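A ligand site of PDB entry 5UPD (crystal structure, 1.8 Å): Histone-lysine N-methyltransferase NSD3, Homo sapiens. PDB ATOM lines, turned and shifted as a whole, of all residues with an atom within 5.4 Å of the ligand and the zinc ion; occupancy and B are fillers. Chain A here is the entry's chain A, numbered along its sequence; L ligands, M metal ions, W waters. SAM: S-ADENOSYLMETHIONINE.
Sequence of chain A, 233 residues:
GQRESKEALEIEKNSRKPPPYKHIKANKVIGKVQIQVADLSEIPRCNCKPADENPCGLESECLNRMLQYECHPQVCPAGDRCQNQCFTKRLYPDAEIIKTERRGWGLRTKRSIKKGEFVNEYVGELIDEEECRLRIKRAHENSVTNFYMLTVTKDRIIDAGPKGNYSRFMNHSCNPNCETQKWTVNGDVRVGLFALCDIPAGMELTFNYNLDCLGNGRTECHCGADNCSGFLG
The backbone NH (N) of Cys 221 lies within hydrogen-bond range of the backbone carbonyl oxygen (O) of Gly 230 (2.8 Å).
The backbone NH (N) of Gly 230 sits close to the side-chain sulfur (SG) of Cys 228.
The backbone NH of Cys 174 is in hydrogen-bond range of a ring nitrogen (NE2) of His 172 (3.5 Å).
N of Ser 229 lies close to SG of Cys 174, at 3.7 Å.
The backbone carbonyl oxygen of Arg 103 is in hydrogen-bond range of the side-chain amide nitrogen of Asn 171.
NE2 of His 222 lies within hydrogen-bond range of OE2 of Glu 220 (3.4 Å).
OH of Tyr 209 sits at hydrogen-bond distance from O of Met 170 (2.8 Å).
The backbone carbonyl oxygen (O) of Thr 219 lies within hydrogen-bond range of the backbone NH (N) of Leu 232 (3.2 Å).
The zinc ion is bound by SG of Cys 221 (2.3 Å), SG of Cys 223 (2.3 Å), SG of Cys 228 (2.3 Å) and SG of Cys 174 (2.4 Å).
The nearest printed residue that does not touch the zinc ion is His 172 (4.3 Å).
O of Arg 168 lies close to SD of the ligand (3.7 Å).
Merely in contact with the ligand: Gly 104 (3.7 Å), Phe 169 (3.7 Å), Met 170 (3.8 Å), Tyr 209 (3.4 Å), Glu 220 (3.4 Å) and Leu 232 (3.5 Å).
Hydrophobic or aromatic side chains within 4 Å of the ligand: Trp 105, Tyr 148, His 172 and Leu 232.
18 residues have an atom within 4 Å of the ligand: Arg 103, Gly 104, Trp 105, Thr 145, Asn 146, Phe 147, Tyr 148, Arg 168, Phe 169, Met 170, Asn 171, His 172, Tyr 209, Glu 220, Cys 221, His 222, Cys 223 and Leu 232.
N6 of the ligand sits close to SG of Cys 221.
The backbone carbonyl oxygen of Arg 103 is in hydrogen-bond range of a nitrogen (N) of the ligand.
OXT of the ligand lies within hydrogen-bond range of OH of Tyr 148, at 2.7 Å.
N of Trp 105 lies within hydrogen-bond range of O of the ligand (2.9 Å).
The backbone carbonyl oxygen (O) of Trp 105 is in hydrogen-bond range of a nitrogen (N) of the ligand (2.8 Å).
A nitrogen (N) of the ligand sits at hydrogen-bond distance from the side-chain amide oxygen of Asn 171, at 2.9 Å.
A nitrogen (N7) of the ligand lies within hydrogen-bond range of the backbone NH (N) of His 172.
O of His 172 lies within hydrogen-bond range of N6 of the ligand (2.9 Å).
N of His 222 is in hydrogen-bond range of N1 of the ligand (3.0 Å).
O of Thr 145 is in hydrogen-bond range of O2' of the ligand (3.0 Å).
The backbone NH (N) of Phe 147 lies within hydrogen-bond range of an oxygen (O3') of the ligand (3.1 Å).
The side-chain amide oxygen of Asn 146 lies close to an oxygen (O2') of the ligand (3.2 Å).
Water W1 bridges O of the ligand (2.8 Å) and ND2 of Asn 146 (3.1 Å).
Water W4 lies within hydrogen-bond range of the side-chain amide oxygen (OD1) of Asn 146 (2.6 Å) and a nitrogen (N) of the ligand (3.0 Å).
Water W2 lies within hydrogen-bond range of the side-chain hydroxyl (OG1) of Thr 145 (2.4 Å), an oxygen (O2') of the ligand (3.2 Å) and the side-chain amide oxygen (OD1) of Asn 146 (3.5 Å).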
ATOM      1  N   ARG A 102       2.461 -20.433   9.659  1.00  0.00           N
ATOM      2  CA  ARG A 102       2.266 -21.851   9.302  1.00  0.00           C
ATOM      3  C   ARG A 102       0.778 -22.284   9.195  1.00  0.00           C
ATOM      4  O   ARG A 102       0.516 -23.417   8.875  1.00  0.00           O
ATOM      5  CB  ARG A 102       2.988 -22.778  10.303  1.00  0.00           C
ATOM      6  CG  ARG A 102       4.497 -22.578  10.379  1.00  0.00           C
ATOM      7  CD  ARG A 102       5.212 -22.993   9.102  1.00  0.00           C
ATOM      8  NE  ARG A 102       4.927 -24.376   8.704  1.00  0.00           N
ATOM      9  CZ  ARG A 102       4.748 -24.767   7.455  1.00  0.00           C
ATOM     10  N   ARG A 103      -0.146 -21.388   9.502  1.00  0.00           N
ATOM     11  CA  ARG A 103      -1.576 -21.704   9.489  1.00  0.00           C
ATOM     12  C   ARG A 103      -2.314 -20.791   8.480  1.00  0.00           C
ATOM     13  O   ARG A 103      -3.534 -20.490   8.678  1.00  0.00           O
ATOM     14  CB  ARG A 103      -2.138 -21.509  10.911  1.00  0.00           C
ATOM     15  CG  ARG A 103      -1.439 -22.388  11.950  1.00  0.00           C
ATOM     16  CD  ARG A 103      -1.852 -22.210  13.428  1.00  0.00           C
ATOM     17  NE  ARG A 103      -1.328 -20.969  13.893  1.00  0.00           N
ATOM     18  CZ  ARG A 103      -2.037 -19.880  14.116  1.00  0.00           C
ATOM     19  NH1 ARG A 103      -3.372 -19.906  14.092  1.00  0.00           N
ATOM     20  NH2 ARG A 103      -1.381 -18.758  14.413  1.00  0.00           N
ATOM     21  N   GLY A 104      -1.584 -20.279   7.470  1.00  0.00           N
ATOM     22  CA  GLY A 104      -2.233 -19.416   6.448  1.00  0.00           C
ATOM     23  C   GLY A 104      -2.757 -18.089   6.993  1.00  0.00           C
ATOM     24  O   GLY A 104      -2.180 -17.475   7.871  1.00  0.00           O
ATOM     25  N   TRP A 105      -3.932 -17.674   6.529  1.00  0.00           N
ATOM     26  CA  TRP A 105      -4.583 -16.480   7.048  1.00  0.00           C
ATOM     27  C   TRP A 105      -5.395 -16.856   8.249  1.00  0.00           C
ATOM     28  O   TRP A 105      -5.930 -17.975   8.319  1.00  0.00           O
ATOM     29  CB  TRP A 105      -5.480 -15.899   5.975  1.00  0.00           C
ATOM     30  CG  TRP A 105      -4.711 -15.615   4.810  1.00  0.00           C
ATOM     31  CD1 TRP A 105      -4.484 -16.461   3.696  1.00  0.00           C
ATOM     32  CD2 TRP A 105      -3.984 -14.445   4.558  1.00  0.00           C
ATOM     33  NE1 TRP A 105      -3.667 -15.848   2.808  1.00  0.00           N
ATOM     34  CE2 TRP A 105      -3.369 -14.596   3.293  1.00  0.00           C
ATOM     35  CE3 TRP A 105      -3.829 -13.259   5.240  1.00  0.00           C
ATOM     36  CZ2 TRP A 105      -2.589 -13.611   2.726  1.00  0.00           C
ATOM     37  CZ3 TRP A 105      -3.046 -12.261   4.670  1.00  0.00           C
ATOM     38  CH2 TRP A 105      -2.450 -12.453   3.425  1.00  0.00           C
ATOM     39  N   GLY A 106      -5.473 -15.976   9.216  1.00  0.00           N
ATOM     40  CA  GLY A 106      -6.358 -16.224  10.373  1.00  0.00           C
ATOM     41  C   GLY A 106      -7.165 -14.991  10.641  1.00  0.00           C
ATOM     42  O   GLY A 106      -7.173 -14.068   9.813  1.00  0.00           O
ATOM     43  N   TYR A 122     -21.235 -18.895  11.410  1.00  0.00           N
ATOM     44  CA  TYR A 122     -20.492 -19.611  10.410  1.00  0.00           C
ATOM     45  C   TYR A 122     -21.444 -19.770   9.236  1.00  0.00           C
ATOM     46  O   TYR A 122     -22.427 -20.495   9.318  1.00  0.00           O
ATOM     47  CB  TYR A 122     -20.017 -20.953  10.933  1.00  0.00           C
ATOM     48  CG  TYR A 122     -18.946 -21.581  10.071  1.00  0.00           C
ATOM     49  CD1 TYR A 122     -17.595 -21.305  10.301  1.00  0.00           C
ATOM     50  CD2 TYR A 122     -19.273 -22.395   8.984  1.00  0.00           C
ATOM     51  CE1 TYR A 122     -16.592 -21.868   9.496  1.00  0.00           C
ATOM     52  CE2 TYR A 122     -18.264 -22.969   8.174  1.00  0.00           C
ATOM     53  CZ  TYR A 122     -16.956 -22.715   8.446  1.00  0.00           C
ATOM     54  OH  TYR A 122     -15.980 -23.218   7.618  1.00  0.00           O
ATOM     55  N   THR A 145      -5.309 -27.547   0.027  1.00  0.00           N
ATOM     56  CA  THR A 145      -5.060 -28.000   1.410  1.00  0.00           C
ATOM     57  C   THR A 145      -5.919 -27.270   2.458  1.00  0.00           C
ATOM     58  O   THR A 145      -5.834 -27.597   3.652  1.00  0.00           O
ATOM     59  CB  THR A 145      -3.577 -27.871   1.780  1.00  0.00           C
ATOM     60  OG1 THR A 145      -3.209 -26.494   1.691  1.00  0.00           O
ATOM     61  CG2 THR A 145      -2.715 -28.658   0.803  1.00  0.00           C
ATOM     62  N   ASN A 146      -6.734 -26.298   2.026  1.00  0.00           N
ATOM     63  CA  ASN A 146      -7.620 -25.544   2.890  1.00  0.00           C
ATOM     64  C   ASN A 146      -9.029 -26.062   2.690  1.00  0.00           C
ATOM     65  O   ASN A 146      -9.535 -26.051   1.568  1.00  0.00           O
ATOM     66  CB  ASN A 146      -7.555 -24.033   2.586  1.00  0.00           C
ATOM     67  CG  ASN A 146      -6.275 -23.388   3.122  1.00  0.00           C
ATOM     68  OD1 ASN A 146      -6.056 -23.329   4.305  1.00  0.00           O
ATOM     69  ND2 ASN A 146      -5.443 -22.891   2.213  1.00  0.00           N
ATOM     70  N   PHE A 147      -9.648 -26.513   3.776  1.00  0.00           N
ATOM     71  CA  PHE A 147     -11.051 -26.945   3.754  1.00  0.00           C
ATOM     72  C   PHE A 147     -11.897 -26.140   4.731  1.00  0.00           C
ATOM     73  O   PHE A 147     -11.421 -25.730   5.786  1.00  0.00           O
ATOM     74  CB  PHE A 147     -11.104 -28.423   4.078  1.00  0.00           C
ATOM     75  CG  PHE A 147     -10.341 -29.259   3.102  1.00  0.00           C
ATOM     76  CD1 PHE A 147     -10.908 -29.633   1.902  1.00  0.00           C
ATOM     77  CD2 PHE A 147      -9.051 -29.584   3.346  1.00  0.00           C
ATOM     78  CE1 PHE A 147     -10.180 -30.352   0.958  1.00  0.00           C
ATOM     79  CE2 PHE A 147      -8.305 -30.324   2.426  1.00  0.00           C
ATOM     80  CZ  PHE A 147      -8.889 -30.721   1.234  1.00  0.00           C
ATOM     81  N   TYR A 148     -13.147 -25.914   4.361  1.00  0.00           N
ATOM     82  CA  TYR A 148     -14.022 -24.986   5.073  1.00  0.00           C
ATOM     83  C   TYR A 148     -15.395 -25.650   5.334  1.00  0.00           C
ATOM     84  O   TYR A 148     -16.391 -24.966   5.490  1.00  0.00           O
ATOM     85  CB  TYR A 148     -14.210 -23.691   4.269  1.00  0.00           C
ATOM     86  CG  TYR A 148     -12.941 -22.952   3.907  1.00  0.00           C
ATOM     87  CD1 TYR A 148     -12.213 -23.331   2.827  1.00  0.00           C
ATOM     88  CD2 TYR A 148     -12.466 -21.898   4.690  1.00  0.00           C
ATOM     89  CE1 TYR A 148     -11.038 -22.694   2.469  1.00  0.00           C
ATOM     90  CE2 TYR A 148     -11.307 -21.216   4.348  1.00  0.00           C
ATOM     91  CZ  TYR A 148     -10.571 -21.627   3.236  1.00  0.00           C
ATOM     92  OH  TYR A 148      -9.360 -21.033   2.845  1.00  0.00           O
ATOM     93  N   ARG A 168     -14.769 -17.863   8.227  1.00  0.00           N
ATOM     94  CA  ARG A 168     -14.043 -18.796   7.435  1.00  0.00           C
ATOM     95  C   ARG A 168     -12.527 -18.750   7.677  1.00  0.00           C
ATOM     96  O   ARG A 168     -11.815 -19.668   7.334  1.00  0.00           O
ATOM     97  CB  ARG A 168     -14.354 -18.608   5.939  1.00  0.00           C
ATOM     98  CG  ARG A 168     -13.569 -17.465   5.292  1.00  0.00           C
ATOM     99  CD  ARG A 168     -14.160 -17.207   3.916  1.00  0.00           C
ATOM    100  NE  ARG A 168     -13.784 -18.205   2.919  1.00  0.00           N
ATOM    101  CZ  ARG A 168     -12.614 -18.298   2.330  1.00  0.00           C
ATOM    102  NH1 ARG A 168     -11.594 -17.530   2.681  1.00  0.00           N
ATOM    103  NH2 ARG A 168     -12.437 -19.161   1.355  1.00  0.00           N
ATOM    104  N   PHE A 169     -12.063 -17.631   8.218  1.00  0.00           N
ATOM    105  CA  PHE A 169     -10.657 -17.462   8.550  1.00  0.00           C
ATOM    106  C   PHE A 169     -10.230 -17.950   9.921  1.00  0.00           C
ATOM    107  O   PHE A 169      -9.039 -17.952  10.200  1.00  0.00           O
ATOM    108  CB  PHE A 169     -10.222 -16.023   8.338  1.00  0.00           C
ATOM    109  CG  PHE A 169     -10.253 -15.580   6.878  1.00  0.00           C
ATOM    110  CD1 PHE A 169      -9.334 -16.097   5.969  1.00  0.00           C
ATOM    111  CD2 PHE A 169     -11.249 -14.769   6.400  1.00  0.00           C
ATOM    112  CE1 PHE A 169      -9.348 -15.718   4.624  1.00  0.00           C
ATOM    113  CE2 PHE A 169     -11.266 -14.371   5.066  1.00  0.00           C
ATOM    114  CZ  PHE A 169     -10.348 -14.866   4.181  1.00  0.00           C
ATOM    115  N   MET A 170     -11.145 -18.409  10.756  1.00  0.00           N
ATOM    116  CA  MET A 170     -10.758 -18.814  12.116  1.00  0.00           C
ATOM    117  C   MET A 170     -10.087 -20.162  12.041  1.00  0.00           C
ATOM    118  O   MET A 170     -10.641 -21.117  11.487  1.00  0.00           O
ATOM    119  CB  MET A 170     -11.996 -18.895  12.994  1.00  0.00           C
ATOM    120  CG  MET A 170     -12.457 -17.514  13.411  1.00  0.00           C
ATOM    121  SD  MET A 170     -14.037 -17.526  14.244  1.00  0.00           S
ATOM    122  CE  MET A 170     -13.564 -18.282  15.785  1.00  0.00           C
ATOM    123  N   ASN A 171      -8.839 -20.203  12.532  1.00  0.00           N
ATOM    124  CA  ASN A 171      -8.066 -21.387  12.548  1.00  0.00           C
ATOM    125  C   ASN A 171      -8.452 -22.353  13.690  1.00  0.00           C
ATOM    126  O   ASN A 171      -9.122 -21.954  14.681  1.00  0.00           O
ATOM    127  CB  ASN A 171      -6.592 -21.016  12.606  1.00  0.00           C
ATOM    128  CG  ASN A 171      -6.077 -20.560  11.274  1.00  0.00           C
ATOM    129  OD1 ASN A 171      -6.417 -21.191  10.236  1.00  0.00           O
ATOM    130  ND2 ASN A 171      -5.170 -19.564  11.278  1.00  0.00           N
ATOM    131  N   HIS A 172      -8.013 -23.602  13.535  1.00  0.00           N
ATOM    132  CA  HIS A 172      -8.157 -24.616  14.546  1.00  0.00           C
ATOM    133  C   HIS A 172      -7.185 -24.447  15.692  1.00  0.00           C
ATOM    134  O   HIS A 172      -6.010 -24.087  15.486  1.00  0.00           O
ATOM    135  CB  HIS A 172      -7.905 -25.998  13.977  1.00  0.00           C
ATOM    136  CG  HIS A 172      -7.748 -27.047  15.040  1.00  0.00           C
ATOM    137  ND1 HIS A 172      -8.831 -27.655  15.639  1.00  0.00           N
ATOM    138  CD2 HIS A 172      -6.641 -27.591  15.599  1.00  0.00           C
ATOM    139  CE1 HIS A 172      -8.382 -28.533  16.527  1.00  0.00           C
ATOM    140  NE2 HIS A 172      -7.059 -28.475  16.545  1.00  0.00           N
ATOM    141  N   SER A 173      -7.648 -24.720  16.913  1.00  0.00           N
ATOM    142  CA  SER A 173      -6.732 -24.837  18.039  1.00  0.00           C
ATOM    143  C   SER A 173      -7.209 -25.983  18.886  1.00  0.00           C
ATOM    144  O   SER A 173      -8.395 -26.172  19.099  1.00  0.00           O
ATOM    145  CB  SER A 173      -6.722 -23.602  18.952  1.00  0.00           C
ATOM    146  OG  SER A 173      -5.849 -23.751  20.057  1.00  0.00           O
ATOM    147  N   CYS A 174      -6.207 -26.680  19.396  1.00  0.00           N
ATOM    148  CA  CYS A 174      -6.401 -27.683  20.399  1.00  0.00           C
ATOM    149  C   CYS A 174      -6.763 -27.088  21.788  1.00  0.00           C
ATOM    150  O   CYS A 174      -7.280 -27.837  22.634  1.00  0.00           O
ATOM    151  CB  CYS A 174      -5.129 -28.553  20.461  1.00  0.00           C
ATOM    152  SG  CYS A 174      -4.773 -29.428  18.931  1.00  0.00           S
ATOM    153  N   TYR A 209     -11.916 -27.628  15.537  1.00  0.00           N
ATOM    154  CA  TYR A 209     -12.594 -28.203  14.352  1.00  0.00           C
ATOM    155  C   TYR A 209     -13.060 -29.648  14.652  1.00  0.00           C
ATOM    156  O   TYR A 209     -12.501 -30.325  15.524  1.00  0.00           O
ATOM    157  CB  TYR A 209     -11.625 -28.309  13.200  1.00  0.00           C
ATOM    158  CG  TYR A 209     -11.174 -27.023  12.562  1.00  0.00           C
ATOM    159  CD1 TYR A 209     -11.461 -25.750  13.111  1.00  0.00           C
ATOM    160  CD2 TYR A 209     -10.446 -27.093  11.419  1.00  0.00           C
ATOM    161  CE1 TYR A 209     -10.989 -24.563  12.462  1.00  0.00           C
ATOM    162  CE2 TYR A 209      -9.985 -25.956  10.798  1.00  0.00           C
ATOM    163  CZ  TYR A 209     -10.243 -24.686  11.335  1.00  0.00           C
ATOM    164  OH  TYR A 209      -9.771 -23.624  10.648  1.00  0.00           O
ATOM    165  N   THR A 219      -4.131 -33.214   8.782  1.00  0.00           N
ATOM    166  CA  THR A 219      -3.258 -32.073   8.509  1.00  0.00           C
ATOM    167  C   THR A 219      -2.520 -31.875   9.812  1.00  0.00           C
ATOM    168  O   THR A 219      -3.134 -31.844  10.868  1.00  0.00           O
ATOM    169  CB  THR A 219      -4.132 -30.850   8.187  1.00  0.00           C
ATOM    170  OG1 THR A 219      -4.715 -31.031   6.902  1.00  0.00           O
ATOM    171  CG2 THR A 219      -3.387 -29.530   8.222  1.00  0.00           C
ATOM    172  N   GLU A 220      -1.220 -31.716   9.738  1.00  0.00           N
ATOM    173  CA  GLU A 220      -0.437 -31.420  10.914  1.00  0.00           C
ATOM    174  C   GLU A 220      -0.874 -30.062  11.575  1.00  0.00           C
ATOM    175  O   GLU A 220      -1.014 -29.047  10.900  1.00  0.00           O
ATOM    176  CB  GLU A 220       1.024 -31.383  10.497  1.00  0.00           C
ATOM    177  CG  GLU A 220       2.020 -30.921  11.550  1.00  0.00           C
ATOM    178  CD  GLU A 220       3.448 -30.947  11.014  1.00  0.00           C
ATOM    179  OE1 GLU A 220       4.339 -31.403  11.742  1.00  0.00           O
ATOM    180  OE2 GLU A 220       3.679 -30.495   9.863  1.00  0.00           O
ATOM    181  N   CYS A 221      -0.999 -30.050  12.888  1.00  0.00           N
ATOM    182  CA  CYS A 221      -1.423 -28.864  13.646  1.00  0.00           C
ATOM    183  C   CYS A 221      -0.275 -28.040  14.129  1.00  0.00           C
ATOM    184  O   CYS A 221       0.679 -28.562  14.764  1.00  0.00           O
ATOM    185  CB  CYS A 221      -2.249 -29.293  14.862  1.00  0.00           C
ATOM    186  SG  CYS A 221      -3.104 -27.901  15.627  1.00  0.00           S
ATOM    187  N   HIS A 222      -0.324 -26.744  13.844  1.00  0.00           N
ATOM    188  CA  HIS A 222       0.626 -25.802  14.399  1.00  0.00           C
ATOM    189  C   HIS A 222       0.007 -24.827  15.360  1.00  0.00           C
ATOM    190  O   HIS A 222       0.416 -23.669  15.445  1.00  0.00           O
ATOM    191  CB  HIS A 222       1.302 -25.082  13.219  1.00  0.00           C
ATOM    192  CG  HIS A 222       2.069 -26.013  12.337  1.00  0.00           C
ATOM    193  ND1 HIS A 222       3.277 -26.565  12.723  1.00  0.00           N
ATOM    194  CD2 HIS A 222       1.792 -26.498  11.121  1.00  0.00           C
ATOM    195  CE1 HIS A 222       3.709 -27.351  11.748  1.00  0.00           C
ATOM    196  NE2 HIS A 222       2.826 -27.323  10.768  1.00  0.00           N
ATOM    197  N   CYS A 223      -1.012 -25.260  16.135  1.00  0.00           N
ATOM    198  CA  CYS A 223      -1.733 -24.320  17.035  1.00  0.00           C
ATOM    199  C   CYS A 223      -0.886 -23.804  18.193  1.00  0.00           C
ATOM    200  O   CYS A 223      -1.184 -22.755  18.772  1.00  0.00           O
ATOM    201  CB  CYS A 223      -3.040 -24.939  17.547  1.00  0.00           C
ATOM    202  SG  CYS A 223      -2.903 -26.203  18.877  1.00  0.00           S
ATOM    203  N   GLY A 224       0.143 -24.590  18.548  1.00  0.00           N
ATOM    204  CA  GLY A 224       1.073 -24.249  19.619  1.00  0.00           C
ATOM    205  C   GLY A 224       0.611 -24.497  21.041  1.00  0.00           C
ATOM    206  O   GLY A 224       1.369 -24.217  21.975  1.00  0.00           O
ATOM    207  N   ALA A 225      -0.591 -25.050  21.237  1.00  0.00           N
ATOM    208  CA  ALA A 225      -1.089 -25.358  22.599  1.00  0.00           C
ATOM    209  C   ALA A 225      -0.256 -26.423  23.314  1.00  0.00           C
ATOM    210  O   ALA A 225       0.266 -27.343  22.706  1.00  0.00           O
ATOM    211  CB  ALA A 225      -2.520 -25.825  22.532  1.00  0.00           C
ATOM    212  N   CYS A 228      -1.605 -29.798  22.342  1.00  0.00           N
ATOM    213  CA  CYS A 228      -1.758 -30.071  20.943  1.00  0.00           C
ATOM    214  C   CYS A 228      -1.527 -31.561  20.624  1.00  0.00           C
ATOM    215  O   CYS A 228      -0.505 -32.124  20.982  1.00  0.00           O
ATOM    216  CB  CYS A 228      -0.847 -29.166  20.104  1.00  0.00           C
ATOM    217  SG  CYS A 228      -0.977 -29.420  18.334  1.00  0.00           S
ATOM    218  N   SER A 229      -2.511 -32.192  19.984  1.00  0.00           N
ATOM    219  CA  SER A 229      -2.428 -33.575  19.581  1.00  0.00           C
ATOM    220  C   SER A 229      -1.448 -33.793  18.445  1.00  0.00           C
ATOM    221  O   SER A 229      -0.973 -34.880  18.282  1.00  0.00           O
ATOM    222  CB  SER A 229      -3.794 -34.091  19.129  1.00  0.00           C
ATOM    223  OG  SER A 229      -4.225 -33.454  17.961  1.00  0.00           O
ATOM    224  N   GLY A 230      -1.146 -32.739  17.675  1.00  0.00           N
ATOM    225  CA  GLY A 230      -0.383 -32.829  16.440  1.00  0.00           C
ATOM    226  C   GLY A 230      -1.181 -32.774  15.144  1.00  0.00           C
ATOM    227  O   GLY A 230      -0.577 -32.592  14.085  1.00  0.00           O
ATOM    228  N   PHE A 231      -2.505 -32.902  15.200  1.00  0.00           N
ATOM    229  CA  PHE A 231      -3.389 -32.937  14.021  1.00  0.00           C
ATOM    230  C   PHE A 231      -4.666 -32.172  14.257  1.00  0.00           C
ATOM    231  O   PHE A 231      -5.026 -31.999  15.409  1.00  0.00           O
ATOM    232  CB  PHE A 231      -3.749 -34.390  13.683  1.00  0.00           C
ATOM    233  CG  PHE A 231      -2.561 -35.252  13.479  1.00  0.00           C
ATOM    234  CD1 PHE A 231      -2.050 -36.022  14.514  1.00  0.00           C
ATOM    235  CD2 PHE A 231      -1.900 -35.263  12.239  1.00  0.00           C
ATOM    236  CE1 PHE A 231      -0.921 -36.805  14.319  1.00  0.00           C
ATOM    237  CE2 PHE A 231      -0.758 -36.041  12.047  1.00  0.00           C
ATOM    238  CZ  PHE A 231      -0.280 -36.816  13.090  1.00  0.00           C
ATOM    239  N   LEU A 232      -5.375 -31.710  13.205  1.00  0.00           N
ATOM    240  CA  LEU A 232      -6.643 -30.930  13.391  1.00  0.00           C
ATOM    241  C   LEU A 232      -7.828 -31.827  13.618  1.00  0.00           C
ATOM    242  O   LEU A 232      -7.827 -32.961  13.137  1.00  0.00           O
ATOM    243  CB  LEU A 232      -7.048 -30.057  12.201  1.00  0.00           C
ATOM    244  CG  LEU A 232      -6.057 -29.281  11.383  1.00  0.00           C
ATOM    245  CD1 LEU A 232      -6.856 -28.364  10.466  1.00  0.00           C
ATOM    246  CD2 LEU A 232      -5.071 -28.453  12.163  1.00  0.00           C
HETATM  247  N   SAM L   1      -5.905 -20.657   7.440  1.00  0.00           N
HETATM  248  CA  SAM L   1      -7.075 -20.666   6.518  1.00  0.00           C
HETATM  249  C   SAM L   1      -6.838 -19.776   5.288  1.00  0.00           C
HETATM  250  O   SAM L   1      -5.704 -19.370   5.072  1.00  0.00           O
HETATM  251  OXT SAM L   1      -7.782 -19.505   4.495  1.00  0.00           O
HETATM  252  CB  SAM L   1      -8.320 -20.249   7.328  1.00  0.00           C
HETATM  253  CG  SAM L   1      -8.989 -21.455   8.049  1.00  0.00           C
HETATM  254  SD  SAM L   1      -9.641 -22.626   6.980  1.00  0.00           S
HETATM  255  CE  SAM L   1     -11.233 -22.906   7.433  1.00  0.00           C
HETATM  256  C5' SAM L   1      -9.005 -24.129   7.323  1.00  0.00           C
HETATM  257  C4' SAM L   1      -7.580 -24.475   6.853  1.00  0.00           C
HETATM  258  O4' SAM L   1      -6.540 -23.732   7.516  1.00  0.00           O
HETATM  259  C3' SAM L   1      -7.272 -25.927   7.234  1.00  0.00           C
HETATM  260  O3' SAM L   1      -7.835 -26.797   6.242  1.00  0.00           O
HETATM  261  C2' SAM L   1      -5.754 -25.925   7.345  1.00  0.00           C
HETATM  262  O2' SAM L   1      -5.224 -25.893   6.055  1.00  0.00           O
HETATM  263  C1' SAM L   1      -5.473 -24.567   7.949  1.00  0.00           C
HETATM  264  N9  SAM L   1      -5.403 -24.573   9.435  1.00  0.00           N
HETATM  265  C8  SAM L   1      -6.349 -24.119  10.282  1.00  0.00           C
HETATM  266  N7  SAM L   1      -5.951 -24.258  11.602  1.00  0.00           N
HETATM  267  C5  SAM L   1      -4.693 -24.829  11.503  1.00  0.00           C
HETATM  268  C6  SAM L   1      -3.682 -25.265  12.469  1.00  0.00           C
HETATM  269  N6  SAM L   1      -3.946 -25.095  13.729  1.00  0.00           N
HETATM  270  N1  SAM L   1      -2.522 -25.810  12.043  1.00  0.00           N
HETATM  271  C2  SAM L   1      -2.267 -25.945  10.711  1.00  0.00           C
HETATM  272  N3  SAM L   1      -3.137 -25.598   9.746  1.00  0.00           N
HETATM  273  C4  SAM L   1      -4.338 -25.018  10.097  1.00  0.00           C
HETATM  274 ZN    ZN M   1      -2.968 -28.293  17.888  1.00  0.00          ZN
HETATM  275  O   HOH W   1      -3.921 -20.427   3.203  1.00  0.00           O
HETATM  276  O   HOH W   2      -3.165 -25.211   3.760  1.00  0.00           O
HETATM  277  O   HOH W   3      -7.302 -18.098   2.304  1.00  0.00           O
HETATM  278  O   HOH W   4      -4.102 -22.408   5.791  1.00  0.00           O
HETATM  279  O   HOH W   5      -8.994 -28.682   7.676  1.00  0.00           O
HETATM  280  O   HOH W   6      -1.903 -26.302   7.431  1.00  0.00           O
